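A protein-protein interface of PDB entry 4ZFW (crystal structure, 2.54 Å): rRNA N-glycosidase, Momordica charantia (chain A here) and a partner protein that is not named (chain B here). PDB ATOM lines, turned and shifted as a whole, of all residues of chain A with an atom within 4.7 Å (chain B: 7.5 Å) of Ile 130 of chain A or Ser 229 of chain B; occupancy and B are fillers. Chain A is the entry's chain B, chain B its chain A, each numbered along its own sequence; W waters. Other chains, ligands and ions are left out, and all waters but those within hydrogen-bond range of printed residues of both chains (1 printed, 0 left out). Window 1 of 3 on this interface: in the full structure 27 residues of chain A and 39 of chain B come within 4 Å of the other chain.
OG of Ser 229 of chain B is in hydrogen-bond range of O of Ile 130 of chain A, at 2.6 Å. The backbone NH of Val 89 of chain A lies within hydrogen-bond range of the side-chain amide oxygen of Asn 208 of chain B (3.1 Å). OD2 of Asp 228 of chain B sits at hydrogen-bond distance from OG1 of Thr 11 of chain A, at 2.8 Å.
N of Phe 211 of chain B sits at hydrogen-bond distance from O of Asp 228 of chain B (3.0 Å). The side-chain hydroxyl of Tyr 232 of chain B lies within hydrogen-bond range of the side-chain carboxylate of Asp 228 of chain B (3.4 Å). N of Gly 131 of chain A lies within hydrogen-bond range of O of Arg 12 of chain A, at 2.8 Å. O of Tyr 232 of chain B is in hydrogen-bond range of OG1 of Thr 236 of chain B, at 3.5 Å. The backbone carbonyl oxygen (O) of Asn 208 of chain B is in hydrogen-bond range of the side-chain hydroxyl (OH) of Tyr 231 of chain B, 2.6 Å away. The backbone carbonyl oxygen (O) of Gly 226 of chain B sits at hydrogen-bond distance from the side-chain hydroxyl (OH) of Tyr 232 of chain B, at 3.5 Å.
Phe 49 of chain A touches Leu 207 of chain B (O to CD2, 3.9 Å). OH of Tyr 231 of chain B touches CG1 of Val 89 of chain A, 3.3 Å away. Arg 129 of chain A touches Tyr 231 of chain B (CG to O, 3.8 Å). Arg 129 of chain A touches Tyr 232 of chain B (CD to CE2, 3.9 Å). CG2 of Val 210 of chain B touches CG2 of Ile 130 of chain A (3.7 Å). Ile 130 of chain A touches Tyr 231 of chain B. Asp 228 of chain B touches Gly 131 of chain A (OD1 to CA, 3.3 Å). Tyr 232 of chain B touches Gly 131 of chain A.
Printed residues of chain B within 4 Å of Ile 130 of chain A: Val 210 (3.7 Å), Ser 229 (2.6 Å) and Tyr 231 (3.8 Å). Ser 229 of chain B touches one residue of chain A. Printed residues of chain B within 4 Å of Thr 11 of chain A: Asp 228 (2.8 Å). Printed residues of chain B within 4 Å of Val 89 of chain A: Asn 208 (3.1 Å) and Tyr 231 (3.3 Å). Of the printed residues of chain A, Asn 208 of chain B touches Val 89 (3.1 Å). Of the printed residues of chain A, Val 210 of chain B touches Ile 130 (3.7 Å). Of the printed residues of chain A, Tyr 231 of chain B touches Val 89, Arg 129 and Ile 130. Gly 226 of chain B touches none of the printed residues of chain A.
Of the 22 printed residues of chain B, 7 touch a printed residue of chain A. Hydrophobic or aromatic side chains of chain B within 4 Å of the printed part of chain A: Leu 207, Val 210, Tyr 231 and Tyr 232. Printed residues of chain A that touch a printed residue of chain B: Thr 11, Phe 49, Val 89, Arg 129, Ile 130 and Gly 131. Hydrophobic or aromatic side chains of chain A that line the printed part of chain B: Val 89 and Ile 130. Along chain A the printed residues that touch a printed residue of chain B span positions 11 to 131. Among the printed residues, 11 pairs touch across the chains. Among the printed residues, no Asp or Glu carboxylate lies within 4 Å of a Lys or Arg side-chain nitrogen of the other chain.
Water W1 lies within hydrogen-bond range of NE of Arg 129 of chain A (2.7 Å) and O of Tyr 231 of chain B (2.9 Å).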
ATOM      1  N   THR A  11      28.483 -30.394  24.125  1.00  0.00           N
ATOM      2  CA  THR A  11      28.797 -29.050  23.707  1.00  0.00           C
ATOM      3  C   THR A  11      28.255 -28.054  24.740  1.00  0.00           C
ATOM      4  O   THR A  11      27.743 -28.452  25.779  1.00  0.00           O
ATOM      5  CB  THR A  11      28.299 -28.814  22.243  1.00  0.00           C
ATOM      6  OG1 THR A  11      28.714 -27.529  21.775  1.00  0.00           O
ATOM      7  CG2 THR A  11      26.809 -28.928  22.127  1.00  0.00           C
ATOM      8  N   ARG A  12      28.463 -26.769  24.495  1.00  0.00           N
ATOM      9  CA  ARG A  12      27.882 -25.702  25.321  1.00  0.00           C
ATOM     10  C   ARG A  12      26.773 -25.069  24.520  1.00  0.00           C
ATOM     11  O   ARG A  12      26.630 -25.329  23.323  1.00  0.00           O
ATOM     12  CB  ARG A  12      28.941 -24.681  25.770  1.00  0.00           C
ATOM     13  CG  ARG A  12      30.066 -25.399  26.514  1.00  0.00           C
ATOM     14  CD  ARG A  12      31.030 -24.479  27.246  1.00  0.00           C
ATOM     15  NE  ARG A  12      31.983 -23.854  26.333  1.00  0.00           N
ATOM     16  CZ  ARG A  12      32.854 -22.912  26.675  1.00  0.00           C
ATOM     17  NH1 ARG A  12      32.915 -22.465  27.939  1.00  0.00           N
ATOM     18  NH2 ARG A  12      33.677 -22.413  25.748  1.00  0.00           N
ATOM     19  N   ILE A  13      25.971 -24.279  25.205  1.00  0.00           N
ATOM     20  CA  ILE A  13      24.960 -23.481  24.593  1.00  0.00           C
ATOM     21  C   ILE A  13      25.163 -22.075  25.083  1.00  0.00           C
ATOM     22  O   ILE A  13      25.034 -21.823  26.285  1.00  0.00           O
ATOM     23  CB  ILE A  13      23.572 -23.958  24.985  1.00  0.00           C
ATOM     24  CG1 ILE A  13      23.412 -25.420  24.566  1.00  0.00           C
ATOM     25  CG2 ILE A  13      22.529 -23.082  24.309  1.00  0.00           C
ATOM     26  CD1 ILE A  13      22.083 -26.049  24.909  1.00  0.00           C
ATOM     27  N   PHE A  49      23.821 -33.838  23.418  1.00  0.00           N
ATOM     28  CA  PHE A  49      22.704 -34.051  22.489  1.00  0.00           C
ATOM     29  C   PHE A  49      22.706 -35.477  21.994  1.00  0.00           C
ATOM     30  O   PHE A  49      23.747 -36.077  21.894  1.00  0.00           O
ATOM     31  CB  PHE A  49      22.813 -33.137  21.268  1.00  0.00           C
ATOM     32  CG  PHE A  49      22.654 -31.684  21.572  1.00  0.00           C
ATOM     33  CD1 PHE A  49      23.647 -30.991  22.260  1.00  0.00           C
ATOM     34  CD2 PHE A  49      21.535 -31.004  21.148  1.00  0.00           C
ATOM     35  CE1 PHE A  49      23.500 -29.637  22.535  1.00  0.00           C
ATOM     36  CE2 PHE A  49      21.373 -29.667  21.416  1.00  0.00           C
ATOM     37  CZ  PHE A  49      22.359 -28.973  22.107  1.00  0.00           C
ATOM     38  N   VAL A  89      15.635 -27.621  17.251  1.00  0.00           N
ATOM     39  CA  VAL A  89      16.380 -26.376  17.105  1.00  0.00           C
ATOM     40  C   VAL A  89      16.251 -25.872  15.662  1.00  0.00           C
ATOM     41  O   VAL A  89      16.641 -26.571  14.739  1.00  0.00           O
ATOM     42  CB  VAL A  89      17.869 -26.578  17.455  1.00  0.00           C
ATOM     43  CG1 VAL A  89      18.603 -25.243  17.454  1.00  0.00           C
ATOM     44  CG2 VAL A  89      18.017 -27.296  18.789  1.00  0.00           C
ATOM     45  N   MET A  95      15.350 -22.623  20.111  1.00  0.00           N
ATOM     46  CA  MET A  95      15.305 -23.916  20.776  1.00  0.00           C
ATOM     47  C   MET A  95      13.899 -24.092  21.261  1.00  0.00           C
ATOM     48  O   MET A  95      13.452 -23.348  22.143  1.00  0.00           O
ATOM     49  CB  MET A  95      16.273 -23.941  21.943  1.00  0.00           C
ATOM     50  CG  MET A  95      17.714 -23.826  21.490  1.00  0.00           C
ATOM     51  SD  MET A  95      18.999 -24.090  22.721  1.00  0.00           S
ATOM     52  CE  MET A  95      18.753 -25.833  23.074  1.00  0.00           C
ATOM     53  N   TRP A 128      19.963 -18.735  20.352  1.00  0.00           N
ATOM     54  CA  TRP A 128      21.029 -19.509  20.998  1.00  0.00           C
ATOM     55  C   TRP A 128      22.025 -20.033  19.985  1.00  0.00           C
ATOM     56  O   TRP A 128      21.634 -20.469  18.905  1.00  0.00           O
ATOM     57  CB  TRP A 128      20.399 -20.682  21.773  1.00  0.00           C
ATOM     58  CG  TRP A 128      19.448 -20.142  22.743  1.00  0.00           C
ATOM     59  CD1 TRP A 128      18.118 -19.952  22.566  1.00  0.00           C
ATOM     60  CD2 TRP A 128      19.777 -19.587  24.001  1.00  0.00           C
ATOM     61  NE1 TRP A 128      17.590 -19.341  23.665  1.00  0.00           N
ATOM     62  CE2 TRP A 128      18.595 -19.085  24.554  1.00  0.00           C
ATOM     63  CE3 TRP A 128      20.967 -19.473  24.721  1.00  0.00           C
ATOM     64  CZ2 TRP A 128      18.548 -18.497  25.831  1.00  0.00           C
ATOM     65  CZ3 TRP A 128      20.935 -18.905  25.985  1.00  0.00           C
ATOM     66  CH2 TRP A 128      19.724 -18.417  26.531  1.00  0.00           C
ATOM     67  N   ARG A 129      23.303 -19.956  20.324  1.00  0.00           N
ATOM     68  CA  ARG A 129      24.343 -20.691  19.621  1.00  0.00           C
ATOM     69  C   ARG A 129      24.689 -21.960  20.382  1.00  0.00           C
ATOM     70  O   ARG A 129      25.129 -21.913  21.552  1.00  0.00           O
ATOM     71  CB  ARG A 129      25.596 -19.856  19.446  1.00  0.00           C
ATOM     72  CG  ARG A 129      26.639 -20.564  18.612  1.00  0.00           C
ATOM     73  CD  ARG A 129      28.013 -19.970  18.793  1.00  0.00           C
ATOM     74  NE  ARG A 129      28.050 -18.602  18.287  1.00  0.00           N
ATOM     75  CZ  ARG A 129      29.038 -17.735  18.499  1.00  0.00           C
ATOM     76  NH1 ARG A 129      30.120 -18.048  19.218  1.00  0.00           N
ATOM     77  NH2 ARG A 129      28.932 -16.538  17.981  1.00  0.00           N
ATOM     78  N   ILE A 130      24.496 -23.096  19.717  1.00  0.00           N
ATOM     79  CA  ILE A 130      24.826 -24.392  20.297  1.00  0.00           C
ATOM     80  C   ILE A 130      26.181 -24.690  19.780  1.00  0.00           C
ATOM     81  O   ILE A 130      26.360 -24.795  18.582  1.00  0.00           O
ATOM     82  CB  ILE A 130      23.830 -25.461  19.849  1.00  0.00           C
ATOM     83  CG1 ILE A 130      22.439 -25.008  20.310  1.00  0.00           C
ATOM     84  CG2 ILE A 130      24.225 -26.847  20.396  1.00  0.00           C
ATOM     85  CD1 ILE A 130      21.362 -26.026  20.081  1.00  0.00           C
ATOM     86  N   GLY A 131      27.154 -24.805  20.668  1.00  0.00           N
ATOM     87  CA  GLY A 131      28.540 -24.810  20.226  1.00  0.00           C
ATOM     88  C   GLY A 131      29.524 -24.577  21.343  1.00  0.00           C
ATOM     89  O   GLY A 131      29.284 -23.803  22.232  1.00  0.00           O
ATOM     90  N   LEU B 197      33.409 -30.966   6.693  1.00  0.00           N
ATOM     91  CA  LEU B 197      32.268 -30.118   6.983  1.00  0.00           C
ATOM     92  C   LEU B 197      31.045 -30.640   6.290  1.00  0.00           C
ATOM     93  O   LEU B 197      29.972 -30.569   6.839  1.00  0.00           O
ATOM     94  CB  LEU B 197      32.508 -28.693   6.515  1.00  0.00           C
ATOM     95  CG  LEU B 197      33.506 -27.892   7.338  1.00  0.00           C
ATOM     96  CD1 LEU B 197      33.864 -26.615   6.621  1.00  0.00           C
ATOM     97  CD2 LEU B 197      32.940 -27.565   8.705  1.00  0.00           C
ATOM     98  N   GLN B 200      29.993 -33.634   8.444  1.00  0.00           N
ATOM     99  CA  GLN B 200      29.355 -33.238   9.718  1.00  0.00           C
ATOM    100  C   GLN B 200      27.986 -32.577   9.572  1.00  0.00           C
ATOM    101  O   GLN B 200      27.073 -32.887  10.362  1.00  0.00           O
ATOM    102  CB  GLN B 200      30.231 -32.327  10.575  1.00  0.00           C
ATOM    103  CG  GLN B 200      31.506 -32.934  11.124  1.00  0.00           C
ATOM    104  CD  GLN B 200      31.376 -34.378  11.599  1.00  0.00           C
ATOM    105  OE1 GLN B 200      32.155 -35.282  11.222  1.00  0.00           O
ATOM    106  NE2 GLN B 200      30.376 -34.605  12.429  1.00  0.00           N
ATOM    107  N   LEU B 201      27.862 -31.675   8.593  1.00  0.00           N
ATOM    108  CA  LEU B 201      26.583 -31.006   8.294  1.00  0.00           C
ATOM    109  C   LEU B 201      25.469 -31.953   8.008  1.00  0.00           C
ATOM    110  O   LEU B 201      24.363 -31.769   8.474  1.00  0.00           O
ATOM    111  CB  LEU B 201      26.695 -30.085   7.097  1.00  0.00           C
ATOM    112  CG  LEU B 201      27.170 -28.685   7.449  1.00  0.00           C
ATOM    113  CD1 LEU B 201      27.826 -27.978   6.280  1.00  0.00           C
ATOM    114  CD2 LEU B 201      26.008 -27.857   7.979  1.00  0.00           C
ATOM    115  N   SER B 204      24.745 -33.980  11.029  1.00  0.00           N
ATOM    116  CA  SER B 204      24.157 -33.168  12.102  1.00  0.00           C
ATOM    117  C   SER B 204      22.627 -33.250  12.155  1.00  0.00           C
ATOM    118  O   SER B 204      22.032 -32.843  13.145  1.00  0.00           O
ATOM    119  CB  SER B 204      24.615 -31.696  12.000  1.00  0.00           C
ATOM    120  OG  SER B 204      23.887 -30.952  11.027  1.00  0.00           O
ATOM    121  N   LEU B 207      21.201 -34.913  15.125  1.00  0.00           N
ATOM    122  CA  LEU B 207      21.440 -34.329  16.445  1.00  0.00           C
ATOM    123  C   LEU B 207      21.096 -32.866  16.505  1.00  0.00           C
ATOM    124  O   LEU B 207      21.871 -32.082  17.051  1.00  0.00           O
ATOM    125  CB  LEU B 207      22.900 -34.441  16.879  1.00  0.00           C
ATOM    126  CG  LEU B 207      23.545 -35.791  17.111  1.00  0.00           C
ATOM    127  CD1 LEU B 207      24.989 -35.587  17.565  1.00  0.00           C
ATOM    128  CD2 LEU B 207      22.745 -36.560  18.147  1.00  0.00           C
ATOM    129  N   ASN B 208      19.938 -32.467  15.998  1.00  0.00           N
ATOM    130  CA  ASN B 208      19.497 -31.076  16.184  1.00  0.00           C
ATOM    131  C   ASN B 208      20.561 -30.015  15.745  1.00  0.00           C
ATOM    132  O   ASN B 208      20.688 -28.932  16.376  1.00  0.00           O
ATOM    133  CB  ASN B 208      19.063 -30.858  17.650  1.00  0.00           C
ATOM    134  CG  ASN B 208      17.555 -30.925  17.854  1.00  0.00           C
ATOM    135  OD1 ASN B 208      16.763 -30.531  17.007  1.00  0.00           O
ATOM    136  ND2 ASN B 208      17.155 -31.403  19.016  1.00  0.00           N
ATOM    137  N   GLY B 209      21.330 -30.323  14.683  1.00  0.00           N
ATOM    138  CA  GLY B 209      22.275 -29.365  14.115  1.00  0.00           C
ATOM    139  C   GLY B 209      23.683 -29.499  14.641  1.00  0.00           C
ATOM    140  O   GLY B 209      24.566 -28.750  14.283  1.00  0.00           O
ATOM    141  N   VAL B 210      23.908 -30.504  15.457  1.00  0.00           N
ATOM    142  CA  VAL B 210      25.157 -30.614  16.164  1.00  0.00           C
ATOM    143  C   VAL B 210      26.001 -31.681  15.487  1.00  0.00           C
ATOM    144  O   VAL B 210      25.507 -32.721  15.104  1.00  0.00           O
ATOM    145  CB  VAL B 210      24.896 -30.941  17.648  1.00  0.00           C
ATOM    146  CG1 VAL B 210      26.204 -31.122  18.402  1.00  0.00           C
ATOM    147  CG2 VAL B 210      24.072 -29.846  18.279  1.00  0.00           C
ATOM    148  N   PHE B 211      27.286 -31.413  15.383  1.00  0.00           N
ATOM    149  CA  PHE B 211      28.206 -32.306  14.704  1.00  0.00           C
ATOM    150  C   PHE B 211      28.559 -33.512  15.566  1.00  0.00           C
ATOM    151  O   PHE B 211      28.569 -33.416  16.782  1.00  0.00           O
ATOM    152  CB  PHE B 211      29.498 -31.546  14.362  1.00  0.00           C
ATOM    153  CG  PHE B 211      29.339 -30.498  13.298  1.00  0.00           C
ATOM    154  CD1 PHE B 211      28.083 -30.161  12.752  1.00  0.00           C
ATOM    155  CD2 PHE B 211      30.465 -29.854  12.811  1.00  0.00           C
ATOM    156  CE1 PHE B 211      27.969 -29.208  11.761  1.00  0.00           C
ATOM    157  CE2 PHE B 211      30.360 -28.908  11.811  1.00  0.00           C
ATOM    158  CZ  PHE B 211      29.115 -28.578  11.281  1.00  0.00           C
ATOM    159  N   GLY B 212      28.887 -34.633  14.929  1.00  0.00           N
ATOM    160  CA  GLY B 212      29.627 -35.703  15.608  1.00  0.00           C
ATOM    161  C   GLY B 212      31.084 -35.376  15.933  1.00  0.00           C
ATOM    162  O   GLY B 212      31.677 -36.021  16.744  1.00  0.00           O
ATOM    163  N   ASP B 213      31.686 -34.395  15.286  1.00  0.00           N
ATOM    164  CA  ASP B 213      33.091 -34.058  15.563  1.00  0.00           C
ATOM    165  C   ASP B 213      33.323 -32.591  15.281  1.00  0.00           C
ATOM    166  O   ASP B 213      32.682 -32.057  14.393  1.00  0.00           O
ATOM    167  CB  ASP B 213      34.028 -34.925  14.689  1.00  0.00           C
ATOM    168  CG  ASP B 213      35.290 -35.374  15.449  1.00  0.00           C
ATOM    169  OD1 ASP B 213      35.974 -34.496  16.042  1.00  0.00           O
ATOM    170  OD2 ASP B 213      35.563 -36.609  15.487  1.00  0.00           O
ATOM    171  N   SER B 214      34.216 -31.945  16.028  1.00  0.00           N
ATOM    172  CA  SER B 214      34.537 -30.531  15.788  1.00  0.00           C
ATOM    173  C   SER B 214      35.517 -30.338  14.608  1.00  0.00           C
ATOM    174  O   SER B 214      36.367 -31.190  14.315  1.00  0.00           O
ATOM    175  CB  SER B 214      35.119 -29.872  17.054  1.00  0.00           C
ATOM    176  OG  SER B 214      35.224 -28.448  16.930  1.00  0.00           O
ATOM    177  N   VAL B 215      35.390 -29.193  13.952  1.00  0.00           N
ATOM    178  CA  VAL B 215      36.262 -28.810  12.851  1.00  0.00           C
ATOM    179  C   VAL B 215      36.925 -27.454  13.116  1.00  0.00           C
ATOM    180  O   VAL B 215      36.237 -26.472  13.378  1.00  0.00           O
ATOM    181  CB  VAL B 215      35.446 -28.726  11.547  1.00  0.00           C
ATOM    182  CG1 VAL B 215      36.328 -28.298  10.385  1.00  0.00           C
ATOM    183  CG2 VAL B 215      34.785 -30.066  11.270  1.00  0.00           C
ATOM    184  N   GLY B 226      36.385 -23.511  16.714  1.00  0.00           N
ATOM    185  CA  GLY B 226      35.930 -24.870  16.731  1.00  0.00           C
ATOM    186  C   GLY B 226      34.503 -24.738  16.300  1.00  0.00           C
ATOM    187  O   GLY B 226      33.723 -24.044  16.940  1.00  0.00           O
ATOM    188  N   VAL B 227      34.197 -25.362  15.174  1.00  0.00           N
ATOM    189  CA  VAL B 227      32.871 -25.379  14.630  1.00  0.00           C
ATOM    190  C   VAL B 227      32.400 -26.801  14.873  1.00  0.00           C
ATOM    191  O   VAL B 227      32.881 -27.725  14.217  1.00  0.00           O
ATOM    192  CB  VAL B 227      32.914 -25.056  13.117  1.00  0.00           C
ATOM    193  CG1 VAL B 227      31.515 -25.144  12.483  1.00  0.00           C
ATOM    194  CG2 VAL B 227      33.598 -23.705  12.891  1.00  0.00           C
ATOM    195  N   ASP B 228      31.479 -26.973  15.815  1.00  0.00           N
ATOM    196  CA  ASP B 228      30.994 -28.301  16.184  1.00  0.00           C
ATOM    197  C   ASP B 228      29.509 -28.375  16.055  1.00  0.00           C
ATOM    198  O   ASP B 228      28.862 -29.182  16.705  1.00  0.00           O
ATOM    199  CB  ASP B 228      31.429 -28.645  17.618  1.00  0.00           C
ATOM    200  CG  ASP B 228      30.898 -27.659  18.637  1.00  0.00           C
ATOM    201  OD1 ASP B 228      30.665 -26.488  18.289  1.00  0.00           O
ATOM    202  OD2 ASP B 228      30.686 -28.055  19.792  1.00  0.00           O
ATOM    203  N   SER B 229      28.968 -27.528  15.208  1.00  0.00           N
ATOM    204  CA  SER B 229      27.537 -27.476  14.948  1.00  0.00           C
ATOM    205  C   SER B 229      27.332 -26.616  13.700  1.00  0.00           C
ATOM    206  O   SER B 229      28.287 -26.000  13.193  1.00  0.00           O
ATOM    207  CB  SER B 229      26.798 -26.816  16.105  1.00  0.00           C
ATOM    208  OG  SER B 229      27.032 -25.405  16.099  1.00  0.00           O
ATOM    209  N   MET B 230      26.078 -26.547  13.253  1.00  0.00           N
ATOM    210  CA  MET B 230      25.670 -25.758  12.093  1.00  0.00           C
ATOM    211  C   MET B 230      25.425 -24.265  12.374  1.00  0.00           C
ATOM    212  O   MET B 230      25.026 -23.507  11.469  1.00  0.00           O
ATOM    213  CB  MET B 230      24.419 -26.351  11.492  1.00  0.00           C
ATOM    214  CG  MET B 230      23.170 -26.238  12.343  1.00  0.00           C
ATOM    215  SD  MET B 230      21.712 -26.704  11.378  1.00  0.00           S
ATOM    216  CE  MET B 230      21.483 -25.185  10.446  1.00  0.00           C
ATOM    217  N   TYR B 231      25.697 -23.832  13.603  1.00  0.00           N
ATOM    218  CA  TYR B 231      25.241 -22.549  14.058  1.00  0.00           C
ATOM    219  C   TYR B 231      26.325 -21.495  14.075  1.00  0.00           C
ATOM    220  O   TYR B 231      26.259 -20.550  14.845  1.00  0.00           O
ATOM    221  CB  TYR B 231      24.610 -22.749  15.427  1.00  0.00           C
ATOM    222  CG  TYR B 231      23.504 -23.766  15.372  1.00  0.00           C
ATOM    223  CD1 TYR B 231      22.313 -23.510  14.676  1.00  0.00           C
ATOM    224  CD2 TYR B 231      23.656 -24.999  15.971  1.00  0.00           C
ATOM    225  CE1 TYR B 231      21.289 -24.458  14.633  1.00  0.00           C
ATOM    226  CE2 TYR B 231      22.649 -25.940  15.925  1.00  0.00           C
ATOM    227  CZ  TYR B 231      21.478 -25.666  15.260  1.00  0.00           C
ATOM    228  OH  TYR B 231      20.547 -26.647  15.234  1.00  0.00           O
ATOM    229  N   TYR B 232      27.306 -21.625  13.195  1.00  0.00           N
ATOM    230  CA  TYR B 232      28.352 -20.635  13.058  1.00  0.00           C
ATOM    231  C   TYR B 232      28.200 -19.914  11.720  1.00  0.00           C
ATOM    232  O   TYR B 232      28.261 -20.549  10.672  1.00  0.00           O
ATOM    233  CB  TYR B 232      29.703 -21.312  13.163  1.00  0.00           C
ATOM    234  CG  TYR B 232      29.977 -21.783  14.550  1.00  0.00           C
ATOM    235  CD1 TYR B 232      29.511 -23.021  14.992  1.00  0.00           C
ATOM    236  CD2 TYR B 232      30.702 -21.006  15.437  1.00  0.00           C
ATOM    237  CE1 TYR B 232      29.756 -23.462  16.290  1.00  0.00           C
ATOM    238  CE2 TYR B 232      30.952 -21.429  16.737  1.00  0.00           C
ATOM    239  CZ  TYR B 232      30.476 -22.652  17.162  1.00  0.00           C
ATOM    240  OH  TYR B 232      30.737 -23.103  18.450  1.00  0.00           O
ATOM    241  N   LEU B 235      30.641 -20.630   8.870  1.00  0.00           N
ATOM    242  CA  LEU B 235      30.395 -21.812   8.054  1.00  0.00           C
ATOM    243  C   LEU B 235      29.194 -21.534   7.148  1.00  0.00           C
ATOM    244  O   LEU B 235      29.290 -21.510   5.901  1.00  0.00           O
ATOM    245  CB  LEU B 235      30.104 -23.014   8.948  1.00  0.00           C
ATOM    246  CG  LEU B 235      29.652 -24.214   8.147  1.00  0.00           C
ATOM    247  CD1 LEU B 235      30.732 -24.574   7.142  1.00  0.00           C
ATOM    248  CD2 LEU B 235      29.332 -25.371   9.053  1.00  0.00           C
ATOM    249  N   THR B 236      28.077 -21.270   7.813  1.00  0.00           N
ATOM    250  CA  THR B 236      26.778 -21.105   7.174  1.00  0.00           C
ATOM    251  C   THR B 236      26.704 -19.995   6.108  1.00  0.00           C
ATOM    252  O   THR B 236      26.059 -20.157   5.100  1.00  0.00           O
ATOM    253  CB  THR B 236      25.728 -20.997   8.304  1.00  0.00           C
ATOM    254  OG1 THR B 236      25.754 -22.250   9.001  1.00  0.00           O
ATOM    255  CG2 THR B 236      24.340 -20.787   7.799  1.00  0.00           C
HETATM  256  O   HOH W   1      26.276 -18.015  16.332  1.00  0.00           O
